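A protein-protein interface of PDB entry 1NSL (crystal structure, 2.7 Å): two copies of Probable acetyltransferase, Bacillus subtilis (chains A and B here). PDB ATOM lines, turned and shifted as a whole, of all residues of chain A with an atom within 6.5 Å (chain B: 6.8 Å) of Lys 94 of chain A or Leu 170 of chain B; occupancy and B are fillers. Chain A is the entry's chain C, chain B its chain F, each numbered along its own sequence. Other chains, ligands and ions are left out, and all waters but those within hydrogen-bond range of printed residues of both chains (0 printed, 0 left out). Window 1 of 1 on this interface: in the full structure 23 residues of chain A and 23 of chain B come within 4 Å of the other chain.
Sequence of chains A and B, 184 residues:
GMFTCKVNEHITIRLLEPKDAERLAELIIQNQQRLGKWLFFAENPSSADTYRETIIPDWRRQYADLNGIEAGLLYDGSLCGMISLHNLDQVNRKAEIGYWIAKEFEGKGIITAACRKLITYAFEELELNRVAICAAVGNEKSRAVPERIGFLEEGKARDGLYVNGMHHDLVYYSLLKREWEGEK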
ATOM      1  N   HIS A  86      19.834  10.022  35.168  1.00  0.00           N
ATOM      2  CA  HIS A  86      20.664   8.945  34.667  1.00  0.00           C
ATOM      3  C   HIS A  86      20.055   8.358  33.412  1.00  0.00           C
ATOM      4  O   HIS A  86      19.052   8.823  32.997  1.00  0.00           O
ATOM      5  CB  HIS A  86      20.836   7.886  35.742  1.00  0.00           C
ATOM      6  CG  HIS A  86      19.552   7.407  36.326  1.00  0.00           C
ATOM      7  ND1 HIS A  86      18.885   6.297  35.854  1.00  0.00           N
ATOM      8  CD2 HIS A  86      18.797   7.899  37.329  1.00  0.00           C
ATOM      9  CE1 HIS A  86      17.779   6.119  36.547  1.00  0.00           C
ATOM     10  NE2 HIS A  86      17.681   7.098  37.428  1.00  0.00           N
ATOM     11  N   ASN A  87      20.647   7.319  32.839  1.00  0.00           N
ATOM     12  CA  ASN A  87      20.264   6.794  31.536  1.00  0.00           C
ATOM     13  C   ASN A  87      20.177   7.906  30.551  1.00  0.00           C
ATOM     14  O   ASN A  87      19.185   8.054  29.859  1.00  0.00           O
ATOM     15  CB  ASN A  87      18.947   6.055  31.554  1.00  0.00           C
ATOM     16  CG  ASN A  87      18.963   4.886  32.511  1.00  0.00           C
ATOM     17  OD1 ASN A  87      19.952   4.690  33.239  1.00  0.00           O
ATOM     18  ND2 ASN A  87      17.861   4.107  32.546  1.00  0.00           N
ATOM     19  N   LEU A  88      21.218   8.701  30.482  1.00  0.00           N
ATOM     20  CA  LEU A  88      21.185   9.819  29.592  1.00  0.00           C
ATOM     21  C   LEU A  88      21.446   9.312  28.205  1.00  0.00           C
ATOM     22  O   LEU A  88      22.509   8.816  27.941  1.00  0.00           O
ATOM     23  CB  LEU A  88      22.279  10.765  29.983  1.00  0.00           C
ATOM     24  CG  LEU A  88      22.162  12.224  29.643  1.00  0.00           C
ATOM     25  CD1 LEU A  88      23.231  12.919  30.521  1.00  0.00           C
ATOM     26  CD2 LEU A  88      22.436  12.448  28.164  1.00  0.00           C
ATOM     27  N   ASP A  89      20.483   9.444  27.309  1.00  0.00           N
ATOM     28  CA  ASP A  89      20.623   8.971  25.959  1.00  0.00           C
ATOM     29  C   ASP A  89      20.509  10.204  25.074  1.00  0.00           C
ATOM     30  O   ASP A  89      19.404  10.626  24.725  1.00  0.00           O
ATOM     31  CB  ASP A  89      19.497   7.996  25.736  1.00  0.00           C
ATOM     32  CG  ASP A  89      19.554   7.287  24.418  1.00  0.00           C
ATOM     33  OD1 ASP A  89      20.282   7.709  23.508  1.00  0.00           O
ATOM     34  OD2 ASP A  89      18.843   6.291  24.193  1.00  0.00           O
ATOM     35  N   GLN A  90      21.653  10.807  24.741  1.00  0.00           N
ATOM     36  CA  GLN A  90      21.708  12.018  23.913  1.00  0.00           C
ATOM     37  C   GLN A  90      21.155  11.786  22.535  1.00  0.00           C
ATOM     38  O   GLN A  90      20.614  12.687  21.915  1.00  0.00           O
ATOM     39  CB  GLN A  90      23.138  12.573  23.781  1.00  0.00           C
ATOM     40  CG  GLN A  90      23.491  13.724  24.738  1.00  0.00           C
ATOM     41  CD  GLN A  90      22.456  14.855  24.697  1.00  0.00           C
ATOM     42  OE1 GLN A  90      21.555  14.864  23.839  1.00  0.00           O
ATOM     43  NE2 GLN A  90      22.575  15.798  25.629  1.00  0.00           N
ATOM     44  N   VAL A  91      21.248  10.571  22.046  1.00  0.00           N
ATOM     45  CA  VAL A  91      20.747  10.354  20.706  1.00  0.00           C
ATOM     46  C   VAL A  91      19.260  10.378  20.682  1.00  0.00           C
ATOM     47  O   VAL A  91      18.672  11.011  19.814  1.00  0.00           O
ATOM     48  CB  VAL A  91      21.201   9.038  20.071  1.00  0.00           C
ATOM     49  CG1 VAL A  91      20.926   9.100  18.580  1.00  0.00           C
ATOM     50  CG2 VAL A  91      22.671   8.816  20.341  1.00  0.00           C
ATOM     51  N   ASN A  92      18.617   9.684  21.598  1.00  0.00           N
ATOM     52  CA  ASN A  92      17.162   9.743  21.548  1.00  0.00           C
ATOM     53  C   ASN A  92      16.633  10.939  22.305  1.00  0.00           C
ATOM     54  O   ASN A  92      15.435  11.149  22.415  1.00  0.00           O
ATOM     55  CB  ASN A  92      16.541   8.442  22.027  1.00  0.00           C
ATOM     56  CG  ASN A  92      17.010   7.259  21.225  1.00  0.00           C
ATOM     57  OD1 ASN A  92      16.724   7.126  20.020  1.00  0.00           O
ATOM     58  ND2 ASN A  92      17.756   6.401  21.878  1.00  0.00           N
ATOM     59  N   ARG A  93      17.555  11.702  22.871  1.00  0.00           N
ATOM     60  CA  ARG A  93      17.173  12.927  23.493  1.00  0.00           C
ATOM     61  C   ARG A  93      16.331  12.738  24.745  1.00  0.00           C
ATOM     62  O   ARG A  93      15.432  13.541  25.014  1.00  0.00           O
ATOM     63  CB  ARG A  93      16.398  13.741  22.468  1.00  0.00           C
ATOM     64  CG  ARG A  93      17.254  14.177  21.275  1.00  0.00           C
ATOM     65  CD  ARG A  93      16.527  15.020  20.228  1.00  0.00           C
ATOM     66  NE  ARG A  93      17.521  15.627  19.348  1.00  0.00           N
ATOM     67  CZ  ARG A  93      17.284  16.530  18.400  1.00  0.00           C
ATOM     68  NH1 ARG A  93      18.288  16.985  17.659  1.00  0.00           N
ATOM     69  NH2 ARG A  93      16.058  16.960  18.177  1.00  0.00           N
ATOM     70  N   LYS A  94      16.651  11.718  25.537  1.00  0.00           N
ATOM     71  CA  LYS A  94      15.834  11.418  26.708  1.00  0.00           C
ATOM     72  C   LYS A  94      16.641  10.999  27.910  1.00  0.00           C
ATOM     73  O   LYS A  94      17.824  10.682  27.783  1.00  0.00           O
ATOM     74  CB  LYS A  94      14.934  10.253  26.376  1.00  0.00           C
ATOM     75  CG  LYS A  94      15.655   9.005  26.027  1.00  0.00           C
ATOM     76  CD  LYS A  94      14.661   7.851  25.857  1.00  0.00           C
ATOM     77  CE  LYS A  94      15.387   6.555  25.441  1.00  0.00           C
ATOM     78  NZ  LYS A  94      14.395   5.509  25.232  1.00  0.00           N
ATOM     79  N   ALA A  95      16.016  10.904  29.076  1.00  0.00           N
ATOM     80  CA  ALA A  95      16.799  10.512  30.259  1.00  0.00           C
ATOM     81  C   ALA A  95      15.835  10.084  31.358  1.00  0.00           C
ATOM     82  O   ALA A  95      14.648  10.290  31.203  1.00  0.00           O
ATOM     83  CB  ALA A  95      17.623  11.697  30.711  1.00  0.00           C
ATOM     84  N   GLU A  96      16.293   9.496  32.447  1.00  0.00           N
ATOM     85  CA  GLU A  96      15.397   9.291  33.591  1.00  0.00           C
ATOM     86  C   GLU A  96      15.767  10.007  34.914  1.00  0.00           C
ATOM     87  O   GLU A  96      16.926  10.390  35.113  1.00  0.00           O
ATOM     88  CB  GLU A  96      15.268   7.847  33.859  1.00  0.00           C
ATOM     89  CG  GLU A  96      15.228   7.108  32.558  1.00  0.00           C
ATOM     90  CD  GLU A  96      15.245   5.635  32.789  1.00  0.00           C
ATOM     91  OE1 GLU A  96      15.067   5.240  33.969  1.00  0.00           O
ATOM     92  OE2 GLU A  96      15.444   4.901  31.805  1.00  0.00           O
ATOM     93  N   LEU A 128      16.869  18.025  26.122  1.00  0.00           N
ATOM     94  CA  LEU A 128      16.259  16.725  25.924  1.00  0.00           C
ATOM     95  C   LEU A 128      14.836  16.893  25.531  1.00  0.00           C
ATOM     96  O   LEU A 128      14.226  17.922  25.807  1.00  0.00           O
ATOM     97  CB  LEU A 128      16.205  15.920  27.236  1.00  0.00           C
ATOM     98  CG  LEU A 128      17.571  15.658  27.847  1.00  0.00           C
ATOM     99  CD1 LEU A 128      17.476  14.538  28.806  1.00  0.00           C
ATOM    100  CD2 LEU A 128      18.529  15.334  26.714  1.00  0.00           C
ATOM    101  N   ASN A 129      14.276  15.820  24.988  1.00  0.00           N
ATOM    102  CA  ASN A 129      12.891  15.835  24.569  1.00  0.00           C
ATOM    103  C   ASN A 129      12.013  15.075  25.550  1.00  0.00           C
ATOM    104  O   ASN A 129      10.866  15.430  25.814  1.00  0.00           O
ATOM    105  CB  ASN A 129      12.758  15.263  23.166  1.00  0.00           C
ATOM    106  CG  ASN A 129      11.357  15.327  22.655  1.00  0.00           C
ATOM    107  OD1 ASN A 129      10.698  14.293  22.472  1.00  0.00           O
ATOM    108  ND2 ASN A 129      10.873  16.544  22.424  1.00  0.00           N
ATOM    109  N   ARG A 130      12.568  14.059  26.153  1.00  0.00           N
ATOM    110  CA  ARG A 130      11.742  13.213  26.966  1.00  0.00           C
ATOM    111  C   ARG A 130      12.356  13.120  28.353  1.00  0.00           C
ATOM    112  O   ARG A 130      13.537  13.168  28.503  1.00  0.00           O
ATOM    113  CB  ARG A 130      11.690  11.854  26.258  1.00  0.00           C
ATOM    114  CG  ARG A 130      11.257  10.693  27.097  1.00  0.00           C
ATOM    115  CD  ARG A 130      11.184   9.349  26.367  1.00  0.00           C
ATOM    116  NE  ARG A 130      11.110   8.287  27.380  1.00  0.00           N
ATOM    117  CZ  ARG A 130       9.976   7.809  27.852  1.00  0.00           C
ATOM    118  NH1 ARG A 130       8.834   8.277  27.373  1.00  0.00           N
ATOM    119  NH2 ARG A 130       9.974   6.867  28.777  1.00  0.00           N
ATOM    120  N   VAL A 131      11.588  13.047  29.400  1.00  0.00           N
ATOM    121  CA  VAL A 131      12.222  12.758  30.673  1.00  0.00           C
ATOM    122  C   VAL A 131      11.341  11.732  31.352  1.00  0.00           C
ATOM    123  O   VAL A 131      10.092  11.858  31.291  1.00  0.00           O
ATOM    124  CB  VAL A 131      12.364  13.990  31.497  1.00  0.00           C
ATOM    125  CG1 VAL A 131      12.369  13.654  32.897  1.00  0.00           C
ATOM    126  CG2 VAL A 131      13.669  14.642  31.137  1.00  0.00           C
ATOM    127  N   ALA A 132      11.902  10.674  31.933  1.00  0.00           N
ATOM    128  CA  ALA A 132      10.970   9.743  32.584  1.00  0.00           C
ATOM    129  C   ALA A 132      11.252   9.571  34.039  1.00  0.00           C
ATOM    130  O   ALA A 132      12.342   9.914  34.515  1.00  0.00           O
ATOM    131  CB  ALA A 132      10.968   8.409  31.901  1.00  0.00           C
ATOM    132  N   LEU B  39      16.992  -0.356  15.681  1.00  0.00           N
ATOM    133  CA  LEU B  39      17.486   0.222  16.948  1.00  0.00           C
ATOM    134  C   LEU B  39      19.001   0.283  16.863  1.00  0.00           C
ATOM    135  O   LEU B  39      19.712  -0.142  17.799  1.00  0.00           O
ATOM    136  CB  LEU B  39      17.009  -0.541  18.197  1.00  0.00           C
ATOM    137  CG  LEU B  39      15.596  -0.114  18.632  1.00  0.00           C
ATOM    138  CD1 LEU B  39      14.967  -0.955  19.756  1.00  0.00           C
ATOM    139  CD2 LEU B  39      15.611   1.337  19.011  1.00  0.00           C
ATOM    140  N   CYS B 134      12.557  -4.212  23.067  1.00  0.00           N
ATOM    141  CA  CYS B 134      11.732  -3.151  22.504  1.00  0.00           C
ATOM    142  C   CYS B 134      11.895  -2.847  21.028  1.00  0.00           C
ATOM    143  O   CYS B 134      12.824  -3.306  20.369  1.00  0.00           O
ATOM    144  CB  CYS B 134      11.708  -1.877  23.379  1.00  0.00           C
ATOM    145  SG  CYS B 134      13.223  -0.953  23.394  1.00  0.00           S
ATOM    146  N   ALA B 135      10.953  -2.090  20.490  1.00  0.00           N
ATOM    147  CA  ALA B 135      10.990  -1.797  19.064  1.00  0.00           C
ATOM    148  C   ALA B 135      10.149  -0.618  18.736  1.00  0.00           C
ATOM    149  O   ALA B 135       9.161  -0.363  19.386  1.00  0.00           O
ATOM    150  CB  ALA B 135      10.517  -2.959  18.302  1.00  0.00           C
ATOM    151  N   ALA B 136      10.549   0.132  17.723  1.00  0.00           N
ATOM    152  CA  ALA B 136       9.676   1.204  17.241  1.00  0.00           C
ATOM    153  C   ALA B 136       8.221   0.725  17.089  1.00  0.00           C
ATOM    154  O   ALA B 136       7.933  -0.361  16.584  1.00  0.00           O
ATOM    155  CB  ALA B 136      10.158   1.691  15.964  1.00  0.00           C
ATOM    156  N   VAL B 137       7.298   1.560  17.517  1.00  0.00           N
ATOM    157  CA  VAL B 137       5.904   1.192  17.453  1.00  0.00           C
ATOM    158  C   VAL B 137       5.482   0.645  16.080  1.00  0.00           C
ATOM    159  O   VAL B 137       4.685  -0.300  16.015  1.00  0.00           O
ATOM    160  CB  VAL B 137       5.031   2.379  17.692  1.00  0.00           C
ATOM    161  CG1 VAL B 137       5.029   3.275  16.418  1.00  0.00           C
ATOM    162  CG2 VAL B 137       3.614   1.905  17.960  1.00  0.00           C
ATOM    163  N   GLY B 155       3.971  -1.930  27.766  1.00  0.00           N
ATOM    164  CA  GLY B 155       3.818  -0.477  27.715  1.00  0.00           C
ATOM    165  C   GLY B 155       4.601   0.251  26.612  1.00  0.00           C
ATOM    166  O   GLY B 155       5.440  -0.299  25.919  1.00  0.00           O
ATOM    167  N   LYS B 156       4.310   1.524  26.433  1.00  0.00           N
ATOM    168  CA  LYS B 156       4.964   2.287  25.392  1.00  0.00           C
ATOM    169  C   LYS B 156       5.848   3.347  26.001  1.00  0.00           C
ATOM    170  O   LYS B 156       5.447   3.919  27.002  1.00  0.00           O
ATOM    171  CB  LYS B 156       3.892   2.976  24.526  1.00  0.00           C
ATOM    172  CG  LYS B 156       3.218   2.064  23.470  1.00  0.00           C
ATOM    173  CD  LYS B 156       2.155   2.810  22.692  1.00  0.00           C
ATOM    174  CE  LYS B 156       1.107   1.902  22.016  1.00  0.00           C
ATOM    175  NZ  LYS B 156       0.145   2.724  21.230  1.00  0.00           N
ATOM    176  N   ALA B 157       7.031   3.602  25.439  1.00  0.00           N
ATOM    177  CA  ALA B 157       7.785   4.805  25.824  1.00  0.00           C
ATOM    178  C   ALA B 157       7.454   5.890  24.813  1.00  0.00           C
ATOM    179  O   ALA B 157       7.833   5.750  23.638  1.00  0.00           O
ATOM    180  CB  ALA B 157       9.184   4.549  25.755  1.00  0.00           C
ATOM    181  N   ARG B 158       6.731   6.943  25.223  1.00  0.00           N
ATOM    182  CA  ARG B 158       6.385   8.048  24.294  1.00  0.00           C
ATOM    183  C   ARG B 158       7.647   8.710  23.826  1.00  0.00           C
ATOM    184  O   ARG B 158       8.530   9.007  24.627  1.00  0.00           O
ATOM    185  CB  ARG B 158       5.549   9.108  24.976  1.00  0.00           C
ATOM    186  CG  ARG B 158       4.456   8.553  25.859  1.00  0.00           C
ATOM    187  CD  ARG B 158       3.399   9.567  26.230  1.00  0.00           C
ATOM    188  NE  ARG B 158       3.890  10.530  27.205  1.00  0.00           N
ATOM    189  CZ  ARG B 158       3.696  11.842  27.124  1.00  0.00           C
ATOM    190  NH1 ARG B 158       3.037  12.384  26.079  1.00  0.00           N
ATOM    191  NH2 ARG B 158       4.168  12.629  28.087  1.00  0.00           N
ATOM    192  N   ASP B 159       7.757   8.903  22.522  1.00  0.00           N
ATOM    193  CA  ASP B 159       8.931   9.537  21.919  1.00  0.00           C
ATOM    194  C   ASP B 159      10.270   8.885  22.389  1.00  0.00           C
ATOM    195  O   ASP B 159      11.258   9.567  22.667  1.00  0.00           O
ATOM    196  CB  ASP B 159       8.920  11.035  22.211  1.00  0.00           C
ATOM    197  CG  ASP B 159       7.725  11.747  21.618  1.00  0.00           C
ATOM    198  OD1 ASP B 159       6.706  11.115  21.223  1.00  0.00           O
ATOM    199  OD2 ASP B 159       7.722  12.980  21.502  1.00  0.00           O
ATOM    200  N   GLY B 160      10.280   7.559  22.477  1.00  0.00           N
ATOM    201  CA  GLY B 160      11.452   6.836  22.912  1.00  0.00           C
ATOM    202  C   GLY B 160      12.525   6.747  21.838  1.00  0.00           C
ATOM    203  O   GLY B 160      13.691   6.501  22.135  1.00  0.00           O
ATOM    204  N   LEU B 161      12.148   6.985  20.587  1.00  0.00           N
ATOM    205  CA  LEU B 161      13.124   6.893  19.524  1.00  0.00           C
ATOM    206  C   LEU B 161      13.389   8.186  18.861  1.00  0.00           C
ATOM    207  O   LEU B 161      12.549   9.072  18.858  1.00  0.00           O
ATOM    208  CB  LEU B 161      12.622   5.968  18.446  1.00  0.00           C
ATOM    209  CG  LEU B 161      13.438   4.692  18.298  1.00  0.00           C
ATOM    210  CD1 LEU B 161      12.742   3.806  17.277  1.00  0.00           C
ATOM    211  CD2 LEU B 161      14.902   4.975  17.884  1.00  0.00           C
ATOM    212  N   HIS B 168       9.598   8.620  17.501  1.00  0.00           N
ATOM    213  CA  HIS B 168       8.540   7.623  17.463  1.00  0.00           C
ATOM    214  C   HIS B 168       8.424   6.954  18.773  1.00  0.00           C
ATOM    215  O   HIS B 168       9.320   7.035  19.588  1.00  0.00           O
ATOM    216  CB  HIS B 168       8.827   6.583  16.422  1.00  0.00           C
ATOM    217  CG  HIS B 168       9.241   7.173  15.126  1.00  0.00           C
ATOM    218  ND1 HIS B 168       8.381   7.899  14.340  1.00  0.00           N
ATOM    219  CD2 HIS B 168      10.437   7.187  14.500  1.00  0.00           C
ATOM    220  CE1 HIS B 168       9.027   8.319  13.269  1.00  0.00           C
ATOM    221  NE2 HIS B 168      10.271   7.884  13.331  1.00  0.00           N
ATOM    222  N   ASP B 169       7.322   6.279  18.986  1.00  0.00           N
ATOM    223  CA  ASP B 169       7.157   5.616  20.249  1.00  0.00           C
ATOM    224  C   ASP B 169       7.897   4.273  20.260  1.00  0.00           C
ATOM    225  O   ASP B 169       8.125   3.663  19.212  1.00  0.00           O
ATOM    226  CB  ASP B 169       5.671   5.430  20.559  1.00  0.00           C
ATOM    227  CG  ASP B 169       4.942   6.759  20.708  1.00  0.00           C
ATOM    228  OD1 ASP B 169       5.641   7.806  20.637  1.00  0.00           O
ATOM    229  OD2 ASP B 169       3.688   6.853  20.865  1.00  0.00           O
ATOM    230  N   LEU B 170       8.286   3.827  21.449  1.00  0.00           N
ATOM    231  CA  LEU B 170       8.856   2.487  21.602  1.00  0.00           C
ATOM    232  C   LEU B 170       7.799   1.625  22.236  1.00  0.00           C
ATOM    233  O   LEU B 170       7.141   2.066  23.177  1.00  0.00           O
ATOM    234  CB  LEU B 170      10.024   2.519  22.556  1.00  0.00           C
ATOM    235  CG  LEU B 170      11.339   2.987  22.015  1.00  0.00           C
ATOM    236  CD1 LEU B 170      12.438   2.903  23.110  1.00  0.00           C
ATOM    237  CD2 LEU B 170      11.669   2.150  20.781  1.00  0.00           C
ATOM    238  N   VAL B 171       7.613   0.421  21.735  1.00  0.00           N
ATOM    239  CA  VAL B 171       6.741  -0.515  22.445  1.00  0.00           C
ATOM    240  C   VAL B 171       7.641  -1.525  23.201  1.00  0.00           C
ATOM    241  O   VAL B 171       8.714  -1.842  22.708  1.00  0.00           O
ATOM    242  CB  VAL B 171       5.817  -1.200  21.494  1.00  0.00           C
ATOM    243  CG1 VAL B 171       6.623  -1.702  20.368  1.00  0.00           C
ATOM    244  CG2 VAL B 171       5.109  -2.321  22.169  1.00  0.00           C
ATOM    245  N   TYR B 172       7.240  -1.967  24.406  1.00  0.00           N
ATOM    246  CA  TYR B 172       8.083  -2.835  25.274  1.00  0.00           C
ATOM    247  C   TYR B 172       7.452  -4.190  25.579  1.00  0.00           C
ATOM    248  O   TYR B 172       6.303  -4.272  26.050  1.00  0.00           O
ATOM    249  CB  TYR B 172       8.421  -2.167  26.620  1.00  0.00           C
ATOM    250  CG  TYR B 172       9.621  -1.215  26.621  1.00  0.00           C
ATOM    251  CD1 TYR B 172       9.438   0.139  26.366  1.00  0.00           C
ATOM    252  CD2 TYR B 172      10.916  -1.649  26.858  1.00  0.00           C
ATOM    253  CE1 TYR B 172      10.455   1.028  26.329  1.00  0.00           C
ATOM    254  CE2 TYR B 172      11.992  -0.717  26.830  1.00  0.00           C
ATOM    255  CZ  TYR B 172      11.721   0.624  26.567  1.00  0.00           C
ATOM    256  OH  TYR B 172      12.689   1.616  26.533  1.00  0.00           O
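Of the 17 printed residues of chain B, 6 touch a printed residue of chain A. Hydrophobic or aromatic side chains of chain B that line the printed part of chain A: Ala 157, Leu 161 and Leu 170. Along chain B the printed residues that touch a printed residue of chain A span positions 157 to 170. Printed residues of chain A that touch a printed residue of chain B: Asn 92, Lys 94, Asn 129 and Arg 130. Among the printed residues, 8 pairs touch across the chains.
Of chain B, only Gly 160 (3.3 Å) and Leu 170 (3.9 Å) come within 4 Å of Lys 94 of chain A. Of the printed residues of chain B, Asn 129 of chain A touches Asp 159. Printed residues of chain B within 4 Å of Arg 130 of chain A: Ala 157, Arg 158 and Asp 159. Of the printed residues of chain A, Ala 157 of chain B touches Arg 130 (3.8 Å). Of the printed residues of chain A, Gly 160 of chain B touches Asn 92 (3.4 Å) and Lys 94 (3.3 Å). Of the printed residues of chain A, Leu 170 of chain B touches Lys 94 (3.9 Å). The nearest printed residue of chain B that does not touch Arg 130 of chain A is Gly 160 of chain B (4.3 Å).
No position is printed for both chains. Of the 8 pairs that touch across the chains among the printed residues, none has its exchanged pair printed and touching as well.
The backbone NH (N) of Leu 161 of chain B is in hydrogen-bond range of the backbone carbonyl oxygen (O) of His 168 of chain B (3.0 Å). The backbone NH of Asp 89 of chain A is in hydrogen-bond range of the backbone carbonyl oxygen of Lys 94 of chain A (3.0 Å). The backbone carbonyl oxygen (O) of Arg 93 of chain A lies within hydrogen-bond range of the backbone NH (N) of Asn 129 of chain A (2.6 Å). The backbone carbonyl oxygen of Arg 130 of chain A is in hydrogen-bond range of the backbone NH of Ala 95 of chain A (3.4 Å). The backbone NH (N) of Asp 159 of chain B lies within hydrogen-bond range of the side-chain carboxylate (OD1) of Asp 169 of chain B, at 3.0 Å. The side-chain amide nitrogen (ND2) of Asn 92 of chain A sits at hydrogen-bond distance from the side-chain carboxylate (OD2) of Asp 89 of chain A (2.6 Å).
The side-chain carboxylate (OD2) of Asp 159 of chain B sits close to the side-chain amide oxygen (OD1) of Asn 129 of chain A (3.4 Å). The guanidinium group (NH1) of Arg 130 of chain A is in hydrogen-bond range of the backbone carbonyl oxygen (O) of Arg 158 of chain B (2.9 Å). O of Gly 160 of chain B is in hydrogen-bond range of NZ of Lys 94 of chain A, 3.3 Å away.
Among the printed residues, merely in contact across the chains: Asn 92 of chain A with Gly 160 of chain B (3.4 Å), Asn 92 of chain A with Leu 161 of chain B (3.5 Å), Lys 94 of chain A with Leu 170 of chain B (3.9 Å), Arg 130 of chain A with Ala 157 of chain B (3.8 Å) and Arg 130 of chain A with Asp 159 of chain B (3.7 Å).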
